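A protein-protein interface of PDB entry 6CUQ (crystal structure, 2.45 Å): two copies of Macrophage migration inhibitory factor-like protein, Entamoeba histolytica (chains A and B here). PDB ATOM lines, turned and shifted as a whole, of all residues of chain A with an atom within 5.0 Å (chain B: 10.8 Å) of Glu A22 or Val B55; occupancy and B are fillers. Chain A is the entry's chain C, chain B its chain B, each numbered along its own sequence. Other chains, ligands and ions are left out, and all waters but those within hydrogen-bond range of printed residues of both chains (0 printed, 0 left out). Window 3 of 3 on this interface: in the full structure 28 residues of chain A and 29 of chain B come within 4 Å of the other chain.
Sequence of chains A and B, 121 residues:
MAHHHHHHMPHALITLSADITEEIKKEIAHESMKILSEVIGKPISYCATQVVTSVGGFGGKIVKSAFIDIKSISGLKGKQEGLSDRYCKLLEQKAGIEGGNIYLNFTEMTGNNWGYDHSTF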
ATOM      1  N   ILE A  20      41.996  -5.995 -34.546  1.00  0.00           N
ATOM      2  CA  ILE A  20      41.756  -4.722 -33.880  1.00  0.00           C
ATOM      3  C   ILE A  20      41.350  -4.968 -32.430  1.00  0.00           C
ATOM      4  O   ILE A  20      40.927  -6.061 -32.051  1.00  0.00           O
ATOM      5  CB  ILE A  20      40.685  -3.886 -34.619  1.00  0.00           C
ATOM      6  CG1 ILE A  20      39.482  -4.760 -34.984  1.00  0.00           C
ATOM      7  CG2 ILE A  20      41.285  -3.227 -35.878  1.00  0.00           C
ATOM      8  CD1 ILE A  20      38.326  -3.986 -35.563  1.00  0.00           C
ATOM      9  N   THR A  21      41.515  -3.937 -31.605  1.00  0.00           N
ATOM     10  CA  THR A  21      41.142  -4.045 -30.203  1.00  0.00           C
ATOM     11  C   THR A  21      39.627  -4.049 -30.044  1.00  0.00           C
ATOM     12  O   THR A  21      38.879  -3.651 -30.936  1.00  0.00           O
ATOM     13  CB  THR A  21      41.721  -2.888 -29.389  1.00  0.00           C
ATOM     14  OG1 THR A  21      41.119  -1.665 -29.825  1.00  0.00           O
ATOM     15  CG2 THR A  21      43.216  -2.805 -29.559  1.00  0.00           C
ATOM     16  N   GLU A  22      39.180  -4.516 -28.878  1.00  0.00           N
ATOM     17  CA  GLU A  22      37.764  -4.424 -28.545  1.00  0.00           C
ATOM     18  C   GLU A  22      37.324  -2.966 -28.450  1.00  0.00           C
ATOM     19  O   GLU A  22      36.213  -2.610 -28.860  1.00  0.00           O
ATOM     20  CB  GLU A  22      37.486  -5.175 -27.243  1.00  0.00           C
ATOM     21  CG  GLU A  22      37.819  -6.664 -27.311  1.00  0.00           C
ATOM     22  CD  GLU A  22      37.113  -7.397 -28.462  1.00  0.00           C
ATOM     23  OE1 GLU A  22      35.862  -7.453 -28.470  1.00  0.00           O
ATOM     24  OE2 GLU A  22      37.810  -7.914 -29.365  1.00  0.00           O
ATOM     25  N   GLU A  23      38.191  -2.104 -27.923  1.00  0.00           N
ATOM     26  CA  GLU A  23      37.866  -0.686 -27.880  1.00  0.00           C
ATOM     27  C   GLU A  23      37.609  -0.137 -29.284  1.00  0.00           C
ATOM     28  O   GLU A  23      36.624   0.579 -29.509  1.00  0.00           O
ATOM     29  CB  GLU A  23      38.987   0.076 -27.173  1.00  0.00           C
ATOM     30  CG  GLU A  23      38.663   1.536 -26.886  1.00  0.00           C
ATOM     31  CD  GLU A  23      37.368   1.695 -26.102  1.00  0.00           C
ATOM     32  OE1 GLU A  23      37.147   0.930 -25.137  1.00  0.00           O
ATOM     33  OE2 GLU A  23      36.570   2.591 -26.448  1.00  0.00           O
ATOM     34  N   ILE A  24      38.463  -0.491 -30.250  1.00  0.00           N
ATOM     35  CA  ILE A  24      38.288   0.006 -31.611  1.00  0.00           C
ATOM     36  C   ILE A  24      36.977  -0.489 -32.202  1.00  0.00           C
ATOM     37  O   ILE A  24      36.282   0.246 -32.915  1.00  0.00           O
ATOM     38  CB  ILE A  24      39.499  -0.385 -32.481  1.00  0.00           C
ATOM     39  CG1 ILE A  24      40.680   0.541 -32.175  1.00  0.00           C
ATOM     40  CG2 ILE A  24      39.142  -0.372 -33.958  1.00  0.00           C
ATOM     41  CD1 ILE A  24      40.409   1.984 -32.510  1.00  0.00           C
ATOM     42  N   LYS A  25      36.610  -1.736 -31.908  1.00  0.00           N
ATOM     43  CA  LYS A  25      35.331  -2.269 -32.379  1.00  0.00           C
ATOM     44  C   LYS A  25      34.150  -1.473 -31.826  1.00  0.00           C
ATOM     45  O   LYS A  25      33.196  -1.177 -32.554  1.00  0.00           O
ATOM     46  CB  LYS A  25      35.199  -3.739 -32.000  1.00  0.00           C
ATOM     47  CG  LYS A  25      36.045  -4.693 -32.810  1.00  0.00           C
ATOM     48  CD  LYS A  25      35.935  -6.108 -32.207  1.00  0.00           C
ATOM     49  CE  LYS A  25      37.197  -6.943 -32.450  1.00  0.00           C
ATOM     50  NZ  LYS A  25      36.984  -8.372 -32.071  1.00  0.00           N
ATOM     51  N   LYS A  26      34.196  -1.110 -30.541  1.00  0.00           N
ATOM     52  CA  LYS A  26      33.163  -0.237 -29.989  1.00  0.00           C
ATOM     53  C   LYS A  26      33.131   1.101 -30.716  1.00  0.00           C
ATOM     54  O   LYS A  26      32.055   1.669 -30.943  1.00  0.00           O
ATOM     55  CB  LYS A  26      33.403  -0.006 -28.506  1.00  0.00           C
ATOM     56  CG  LYS A  26      33.354  -1.245 -27.669  1.00  0.00           C
ATOM     57  CD  LYS A  26      33.573  -0.875 -26.214  1.00  0.00           C
ATOM     58  CE  LYS A  26      33.927  -2.085 -25.378  1.00  0.00           C
ATOM     59  NZ  LYS A  26      33.825  -1.747 -23.938  1.00  0.00           N
ATOM     60  N   ALA A  29      31.337   0.621 -34.000  1.00  0.00           N
ATOM     61  CA  ALA A  29      29.899   0.554 -33.760  1.00  0.00           C
ATOM     62  C   ALA A  29      29.328   1.925 -33.423  1.00  0.00           C
ATOM     63  O   ALA A  29      28.262   2.303 -33.925  1.00  0.00           O
ATOM     64  CB  ALA A  29      29.607  -0.424 -32.624  1.00  0.00           C
ATOM     65  N   THR A  49      23.901  -1.310 -34.378  1.00  0.00           N
ATOM     66  CA  THR A  49      25.049  -1.868 -35.078  1.00  0.00           C
ATOM     67  C   THR A  49      25.643  -3.027 -34.282  1.00  0.00           C
ATOM     68  O   THR A  49      25.732  -2.968 -33.049  1.00  0.00           O
ATOM     69  CB  THR A  49      26.119  -0.796 -35.338  1.00  0.00           C
ATOM     70  OG1 THR A  49      25.605   0.164 -36.265  1.00  0.00           O
ATOM     71  CG2 THR A  49      27.377  -1.404 -35.938  1.00  0.00           C
ATOM     72  N   GLN A  50      26.027  -4.079 -35.003  1.00  0.00           N
ATOM     73  CA  GLN A  50      26.793  -5.196 -34.461  1.00  0.00           C
ATOM     74  C   GLN A  50      28.084  -5.349 -35.254  1.00  0.00           C
ATOM     75  O   GLN A  50      28.053  -5.399 -36.489  1.00  0.00           O
ATOM     76  CB  GLN A  50      25.998  -6.516 -34.517  1.00  0.00           C
ATOM     77  CG  GLN A  50      24.654  -6.482 -33.814  1.00  0.00           C
ATOM     78  CD  GLN A  50      24.800  -6.164 -32.347  1.00  0.00           C
ATOM     79  OE1 GLN A  50      25.826  -6.468 -31.741  1.00  0.00           O
ATOM     80  NE2 GLN A  50      23.789  -5.523 -31.772  1.00  0.00           N
ATOM     81  N   VAL A  51      29.205  -5.452 -34.545  1.00  0.00           N
ATOM     82  CA  VAL A  51      30.522  -5.648 -35.144  1.00  0.00           C
ATOM     83  C   VAL A  51      30.938  -7.089 -34.859  1.00  0.00           C
ATOM     84  O   VAL A  51      31.023  -7.500 -33.696  1.00  0.00           O
ATOM     85  CB  VAL A  51      31.548  -4.640 -34.595  1.00  0.00           C
ATOM     86  CG1 VAL A  51      32.859  -4.758 -35.324  1.00  0.00           C
ATOM     87  CG2 VAL A  51      31.003  -3.212 -34.693  1.00  0.00           C
ATOM     88  N   ILE B  14      21.499 -15.511 -34.882  1.00  0.00           N
ATOM     89  CA  ILE B  14      21.422 -14.598 -33.751  1.00  0.00           C
ATOM     90  C   ILE B  14      22.809 -14.009 -33.553  1.00  0.00           C
ATOM     91  O   ILE B  14      23.774 -14.728 -33.249  1.00  0.00           O
ATOM     92  CB  ILE B  14      20.935 -15.308 -32.483  1.00  0.00           C
ATOM     93  CG1 ILE B  14      19.578 -15.965 -32.748  1.00  0.00           C
ATOM     94  CG2 ILE B  14      20.840 -14.307 -31.326  1.00  0.00           C
ATOM     95  CD1 ILE B  14      19.077 -16.845 -31.619  1.00  0.00           C
ATOM     96  N   THR B  15      22.915 -12.707 -33.766  1.00  0.00           N
ATOM     97  CA  THR B  15      24.136 -11.954 -33.529  1.00  0.00           C
ATOM     98  C   THR B  15      23.880 -11.130 -32.277  1.00  0.00           C
ATOM     99  O   THR B  15      23.028 -10.236 -32.284  1.00  0.00           O
ATOM    100  CB  THR B  15      24.462 -11.080 -34.741  1.00  0.00           C
ATOM    101  OG1 THR B  15      24.501 -11.893 -35.925  1.00  0.00           O
ATOM    102  CG2 THR B  15      25.774 -10.309 -34.552  1.00  0.00           C
ATOM    103  N   LEU B  16      24.566 -11.448 -31.190  1.00  0.00           N
ATOM    104  CA  LEU B  16      24.308 -10.740 -29.947  1.00  0.00           C
ATOM    105  C   LEU B  16      25.611 -10.334 -29.280  1.00  0.00           C
ATOM    106  O   LEU B  16      26.663 -10.945 -29.492  1.00  0.00           O
ATOM    107  CB  LEU B  16      23.450 -11.580 -28.998  1.00  0.00           C
ATOM    108  CG  LEU B  16      24.083 -12.668 -28.141  1.00  0.00           C
ATOM    109  CD1 LEU B  16      23.002 -13.330 -27.305  1.00  0.00           C
ATOM    110  CD2 LEU B  16      24.820 -13.688 -28.969  1.00  0.00           C
ATOM    111  N   SER B  17      25.535  -9.271 -28.482  1.00  0.00           N
ATOM    112  CA  SER B  17      26.719  -8.669 -27.889  1.00  0.00           C
ATOM    113  C   SER B  17      26.727  -8.734 -26.365  1.00  0.00           C
ATOM    114  O   SER B  17      27.354  -7.901 -25.714  1.00  0.00           O
ATOM    115  CB  SER B  17      26.851  -7.216 -28.349  1.00  0.00           C
ATOM    116  OG  SER B  17      25.974  -6.403 -27.598  1.00  0.00           O
ATOM    117  N   ALA B  18      26.061  -9.709 -25.770  1.00  0.00           N
ATOM    118  CA  ALA B  18      26.122  -9.858 -24.325  1.00  0.00           C
ATOM    119  C   ALA B  18      27.363 -10.643 -23.928  1.00  0.00           C
ATOM    120  O   ALA B  18      27.888 -11.448 -24.697  1.00  0.00           O
ATOM    121  CB  ALA B  18      24.872 -10.553 -23.788  1.00  0.00           C
ATOM    122  N   ASP B  19      27.827 -10.403 -22.708  1.00  0.00           N
ATOM    123  CA  ASP B  19      28.927 -11.161 -22.106  1.00  0.00           C
ATOM    124  C   ASP B  19      28.327 -12.406 -21.447  1.00  0.00           C
ATOM    125  O   ASP B  19      27.859 -12.365 -20.309  1.00  0.00           O
ATOM    126  CB  ASP B  19      29.677 -10.262 -21.118  1.00  0.00           C
ATOM    127  CG  ASP B  19      30.718 -11.005 -20.294  1.00  0.00           C
ATOM    128  OD1 ASP B  19      31.322 -11.974 -20.798  1.00  0.00           O
ATOM    129  OD2 ASP B  19      30.916 -10.639 -19.114  1.00  0.00           O
ATOM    130  N   LYS B  25      25.041 -19.729 -24.564  1.00  0.00           N
ATOM    131  CA  LYS B  25      24.875 -19.658 -26.015  1.00  0.00           C
ATOM    132  C   LYS B  25      24.267 -20.946 -26.572  1.00  0.00           C
ATOM    133  O   LYS B  25      23.405 -20.901 -27.460  1.00  0.00           O
ATOM    134  CB  LYS B  25      26.216 -19.381 -26.677  1.00  0.00           C
ATOM    135  CG  LYS B  25      26.657 -17.974 -26.545  1.00  0.00           C
ATOM    136  CD  LYS B  25      28.095 -17.791 -27.009  1.00  0.00           C
ATOM    137  CE  LYS B  25      28.766 -16.600 -26.277  1.00  0.00           C
ATOM    138  NZ  LYS B  25      30.101 -16.238 -26.839  1.00  0.00           N
ATOM    139  N   VAL B  52      26.050 -15.894 -32.810  1.00  0.00           N
ATOM    140  CA  VAL B  52      27.297 -15.211 -33.125  1.00  0.00           C
ATOM    141  C   VAL B  52      27.532 -14.109 -32.093  1.00  0.00           C
ATOM    142  O   VAL B  52      26.663 -13.256 -31.878  1.00  0.00           O
ATOM    143  CB  VAL B  52      27.259 -14.646 -34.558  1.00  0.00           C
ATOM    144  CG1 VAL B  52      28.492 -13.756 -34.855  1.00  0.00           C
ATOM    145  CG2 VAL B  52      27.099 -15.801 -35.572  1.00  0.00           C
ATOM    146  N   THR B  53      28.703 -14.132 -31.459  1.00  0.00           N
ATOM    147  CA  THR B  53      29.074 -13.120 -30.479  1.00  0.00           C
ATOM    148  C   THR B  53      29.619 -11.879 -31.169  1.00  0.00           C
ATOM    149  O   THR B  53      30.596 -11.950 -31.920  1.00  0.00           O
ATOM    150  CB  THR B  53      30.123 -13.664 -29.519  1.00  0.00           C
ATOM    151  OG1 THR B  53      29.541 -14.670 -28.694  1.00  0.00           O
ATOM    152  CG2 THR B  53      30.665 -12.539 -28.632  1.00  0.00           C
ATOM    153  N   SER B  54      29.043 -10.728 -30.850  1.00  0.00           N
ATOM    154  CA  SER B  54      29.412  -9.473 -31.491  1.00  0.00           C
ATOM    155  C   SER B  54      29.759  -8.410 -30.453  1.00  0.00           C
ATOM    156  O   SER B  54      29.653  -8.622 -29.243  1.00  0.00           O
ATOM    157  CB  SER B  54      28.273  -8.961 -32.369  1.00  0.00           C
ATOM    158  OG  SER B  54      27.134  -8.724 -31.562  1.00  0.00           O
ATOM    159  N   VAL B  55      30.220  -7.267 -30.958  1.00  0.00           N
ATOM    160  CA  VAL B  55      30.276  -6.005 -30.225  1.00  0.00           C
ATOM    161  C   VAL B  55      29.178  -5.132 -30.800  1.00  0.00           C
ATOM    162  O   VAL B  55      29.082  -4.991 -32.024  1.00  0.00           O
ATOM    163  CB  VAL B  55      31.649  -5.317 -30.360  1.00  0.00           C
ATOM    164  CG1 VAL B  55      31.577  -3.897 -29.873  1.00  0.00           C
ATOM    165  CG2 VAL B  55      32.703  -6.085 -29.592  1.00  0.00           C
ATOM    166  N   GLY B  56      28.324  -4.584 -29.939  1.00  0.00           N
ATOM    167  CA  GLY B  56      27.071  -4.034 -30.412  1.00  0.00           C
ATOM    168  C   GLY B  56      26.671  -2.740 -29.736  1.00  0.00           C
ATOM    169  O   GLY B  56      27.055  -2.442 -28.607  1.00  0.00           O
ATOM    170  N   GLY B  57      25.810  -2.012 -30.431  1.00  0.00           N
ATOM    171  CA  GLY B  57      25.310  -0.759 -29.912  1.00  0.00           C
ATOM    172  C   GLY B  57      23.883  -0.523 -30.346  1.00  0.00           C
ATOM    173  O   GLY B  57      23.407  -1.072 -31.345  1.00  0.00           O
ATOM    174  N   PHE B  58      23.211   0.324 -29.578  1.00  0.00           N
ATOM    175  CA  PHE B  58      21.835   0.676 -29.867  1.00  0.00           C
ATOM    176  C   PHE B  58      21.627   2.116 -29.444  1.00  0.00           C
ATOM    177  O   PHE B  58      21.996   2.486 -28.327  1.00  0.00           O
ATOM    178  CB  PHE B  58      20.875  -0.252 -29.123  1.00  0.00           C
ATOM    179  CG  PHE B  58      19.705  -0.654 -29.926  1.00  0.00           C
ATOM    180  CD1 PHE B  58      19.709  -1.843 -30.626  1.00  0.00           C
ATOM    181  CD2 PHE B  58      18.593   0.162 -30.000  1.00  0.00           C
ATOM    182  CE1 PHE B  58      18.615  -2.219 -31.374  1.00  0.00           C
ATOM    183  CE2 PHE B  58      17.494  -0.210 -30.754  1.00  0.00           C
ATOM    184  CZ  PHE B  58      17.508  -1.398 -31.443  1.00  0.00           C
ATOM    185  N   LYS B  61      24.617   4.252 -28.170  1.00  0.00           N
ATOM    186  CA  LYS B  61      25.288   3.788 -26.964  1.00  0.00           C
ATOM    187  C   LYS B  61      25.742   2.344 -27.131  1.00  0.00           C
ATOM    188  O   LYS B  61      25.117   1.562 -27.856  1.00  0.00           O
ATOM    189  CB  LYS B  61      24.372   3.895 -25.740  1.00  0.00           C
ATOM    190  CG  LYS B  61      24.087   5.331 -25.290  1.00  0.00           C
ATOM    191  CD  LYS B  61      23.051   5.356 -24.170  1.00  0.00           C
ATOM    192  CE  LYS B  61      22.210   6.634 -24.219  1.00  0.00           C
ATOM    193  NZ  LYS B  61      20.751   6.313 -24.282  1.00  0.00           N
ATOM    194  N   ILE B  62      26.848   2.001 -26.472  1.00  0.00           N
ATOM    195  CA  ILE B  62      27.328   0.622 -26.440  1.00  0.00           C
ATOM    196  C   ILE B  62      26.596  -0.121 -25.328  1.00  0.00           C
ATOM    197  O   ILE B  62      26.783   0.187 -24.148  1.00  0.00           O
ATOM    198  CB  ILE B  62      28.846   0.564 -26.220  1.00  0.00           C
ATOM    199  CG1 ILE B  62      29.579   1.348 -27.301  1.00  0.00           C
ATOM    200  CG2 ILE B  62      29.279  -0.897 -26.260  1.00  0.00           C
ATOM    201  CD1 ILE B  62      29.224   0.915 -28.705  1.00  0.00           C
ATOM    202  N   VAL B  63      25.798  -1.125 -25.694  1.00  0.00           N
ATOM    203  CA  VAL B  63      24.934  -1.804 -24.730  1.00  0.00           C
ATOM    204  C   VAL B  63      24.655  -3.234 -25.201  1.00  0.00           C
ATOM    205  O   VAL B  63      24.834  -3.567 -26.381  1.00  0.00           O
ATOM    206  CB  VAL B  63      23.628  -0.988 -24.515  1.00  0.00           C
ATOM    207  CG1 VAL B  63      22.749  -1.020 -25.761  1.00  0.00           C
ATOM    208  CG2 VAL B  63      22.864  -1.429 -23.264  1.00  0.00           C
ATOM    209  N   LYS B  64      24.249  -4.096 -24.262  1.00  0.00           N
ATOM    210  CA  LYS B  64      23.816  -5.444 -24.616  1.00  0.00           C
ATOM    211  C   LYS B  64      22.705  -5.351 -25.644  1.00  0.00           C
ATOM    212  O   LYS B  64      21.686  -4.696 -25.410  1.00  0.00           O
ATOM    213  CB  LYS B  64      23.250  -6.179 -23.408  1.00  0.00           C
ATOM    214  CG  LYS B  64      24.159  -6.577 -22.308  1.00  0.00           C
ATOM    215  CD  LYS B  64      23.291  -6.692 -21.064  1.00  0.00           C
ATOM    216  CE  LYS B  64      23.986  -7.438 -19.949  1.00  0.00           C
ATOM    217  NZ  LYS B  64      23.211  -7.336 -18.676  1.00  0.00           N
ATOM    218  N   SER B  65      22.885  -6.034 -26.764  1.00  0.00           N
ATOM    219  CA  SER B  65      21.963  -5.883 -27.874  1.00  0.00           C
ATOM    220  C   SER B  65      22.071  -7.118 -28.746  1.00  0.00           C
ATOM    221  O   SER B  65      22.931  -7.971 -28.545  1.00  0.00           O
ATOM    222  CB  SER B  65      22.259  -4.609 -28.683  1.00  0.00           C
ATOM    223  OG  SER B  65      23.636  -4.500 -28.969  1.00  0.00           O
ATOM    224  N   ALA B  66      21.189  -7.193 -29.729  1.00  0.00           N
ATOM    225  CA  ALA B  66      21.178  -8.341 -30.611  1.00  0.00           C
ATOM    226  C   ALA B  66      20.539  -7.940 -31.925  1.00  0.00           C
ATOM    227  O   ALA B  66      19.858  -6.917 -32.021  1.00  0.00           O
ATOM    228  CB  ALA B  66      20.429  -9.530 -29.990  1.00  0.00           C
ATOM    229  N   PHE B  67      20.801  -8.753 -32.943  1.00  0.00           N
ATOM    230  CA  PHE B  67      20.103  -8.718 -34.218  1.00  0.00           C
ATOM    231  C   PHE B  67      19.809 -10.166 -34.589  1.00  0.00           C
ATOM    232  O   PHE B  67      20.723 -10.997 -34.600  1.00  0.00           O
ATOM    233  CB  PHE B  67      20.950  -8.021 -35.289  1.00  0.00           C
ATOM    234  CG  PHE B  67      20.252  -7.859 -36.605  1.00  0.00           C
ATOM    235  CD1 PHE B  67      20.495  -8.731 -37.653  1.00  0.00           C
ATOM    236  CD2 PHE B  67      19.358  -6.819 -36.795  1.00  0.00           C
ATOM    237  CE1 PHE B  67      19.843  -8.578 -38.864  1.00  0.00           C
ATOM    238  CE2 PHE B  67      18.711  -6.648 -38.004  1.00  0.00           C
ATOM    239  CZ  PHE B  67      18.954  -7.526 -39.039  1.00  0.00           C
ATOM    240  N   ILE B  97      19.347  -8.950 -22.188  1.00  0.00           N
ATOM    241  CA  ILE B  97      19.231  -7.946 -23.236  1.00  0.00           C
ATOM    242  C   ILE B  97      17.809  -7.401 -23.232  1.00  0.00           C
ATOM    243  O   ILE B  97      16.833  -8.166 -23.184  1.00  0.00           O
ATOM    244  CB  ILE B  97      19.615  -8.539 -24.604  1.00  0.00           C
ATOM    245  CG1 ILE B  97      21.016  -9.168 -24.531  1.00  0.00           C
ATOM    246  CG2 ILE B  97      19.548  -7.486 -25.677  1.00  0.00           C
ATOM    247  CD1 ILE B  97      21.486  -9.801 -25.830  1.00  0.00           C
ATOM    248  N   ASN B 101      16.570  -3.203 -27.249  1.00  0.00           N
ATOM    249  CA  ASN B 101      17.900  -3.306 -27.833  1.00  0.00           C
ATOM    250  C   ASN B 101      18.042  -4.566 -28.688  1.00  0.00           C
ATOM    251  O   ASN B 101      19.142  -5.093 -28.861  1.00  0.00           O
ATOM    252  CB  ASN B 101      18.967  -3.270 -26.739  1.00  0.00           C
ATOM    253  CG  ASN B 101      18.982  -1.964 -25.991  1.00  0.00           C
ATOM    254  OD1 ASN B 101      18.656  -0.912 -26.546  1.00  0.00           O
ATOM    255  ND2 ASN B 101      19.364  -2.015 -24.723  1.00  0.00           N
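Val B55 touches just these residues of chain A: Glu A22 (3.6 Å), Lys A26 (3.9 Å), Gln A50 (3.3 Å) and Val A51 (2.6 Å).
No residue of chain B comes within 4 Å of Thr A21.
No residue of chain B comes within 4 Å of Glu A23.
No residue of chain B comes within 4 Å of Lys A25.
Lys A26 touches just these residues of chain B: Val B55 (3.9 Å) and Ile B62 (3.7 Å).
Of chain B, only Thr B15 (3.8 Å), Ser B17 (3.6 Å), Ser B54 (2.6 Å), Val B55 (3.3 Å), Gly B56 (3.0 Å), Ser B65 (3.0 Å) and Ala B66 (3.7 Å) come within 4 Å of Gln A50.
Of chain B, only Ser B54 (3.4 Å) and Val B55 (2.6 Å) come within 4 Å of Val A51.
Of the printed residues of chain A, Ser B65 touches Gln A50 (3.0 Å).
Printed residues of chain A within 4 Å of Gly B56: Thr A49 (3.1 Å) and Gln A50 (3.0 Å).
Printed residues of chain A within 4 Å of Thr B15: Gln A50 (3.8 Å).
Lys B64 touches none of the printed residues of chain A.
The nearest residue of chain B that does not touch Glu A22 is Ser B54 (6.4 Å).
The nearest printed residue of chain A that does not touch Val B55 is Lys A25 (4.04 Å).
The nearest printed residue of chain A that does not touch Ser B65 is Thr A49 (4.8 Å).
Of the 23 printed residues of chain B, 9 touch a printed residue of chain A.
Hydrophobic or aromatic side chains of chain A within 4 Å of the printed part of chain B: Val A51.
Among the printed residues, 14 pairs touch across the chains.
Among the printed residues, no Asp or Glu carboxylate lies within 4 Å of a Lys or Arg side-chain nitrogen of the other chain.
The side-chain amide nitrogen (NE2) of Gln A50 sits at hydrogen-bond distance from the side-chain hydroxyl (OG) of Ser B65 (3.0 Å).
The side-chain hydroxyl of Ser B54 lies within hydrogen-bond range of the side-chain amide oxygen of Gln A50.
N of Val A51 sits at hydrogen-bond distance from O of Val B55, at 2.6 Å.
The backbone NH of Gly B57 lies within hydrogen-bond range of the backbone carbonyl oxygen of Thr A49.
Position printed for both chains: 25.
Among the printed residues, pairs that only touch across the chains: Gln A50 with Gly B56, Thr A49 with Gly B56, Gln A50 with Val B55, Val A51 with Ser B54, Glu A22 with Val B55, Gln A50 with Ser B17, Lys A26 with Ile B62, Gln A50 with Ala B66, Gln A50 with Thr B15 and Lys A26 with Val B55.
The backbone NH of Ser B17 sits at hydrogen-bond distance from the backbone carbonyl oxygen of Ser B65.
The backbone NH (N) of Val B63 sits at hydrogen-bond distance from the backbone carbonyl oxygen (O) of Gly B56 (3.4 Å).
The side-chain amino group (NZ) of Lys A25 lies within salt-bridge range of the side-chain carboxylate (OE2) of Glu A22 (2.9 Å).
The backbone carbonyl oxygen (O) of Asn B101 lies within hydrogen-bond range of the backbone NH (N) of Ala B66 (3.1 Å).
OG of Ser B65 lies within hydrogen-bond range of O of Val B63, 3.0 Å away.
The side-chain hydroxyl (OG) of Ser B17 lies within hydrogen-bond range of the backbone carbonyl oxygen (O) of Val B63 (3.3 Å).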
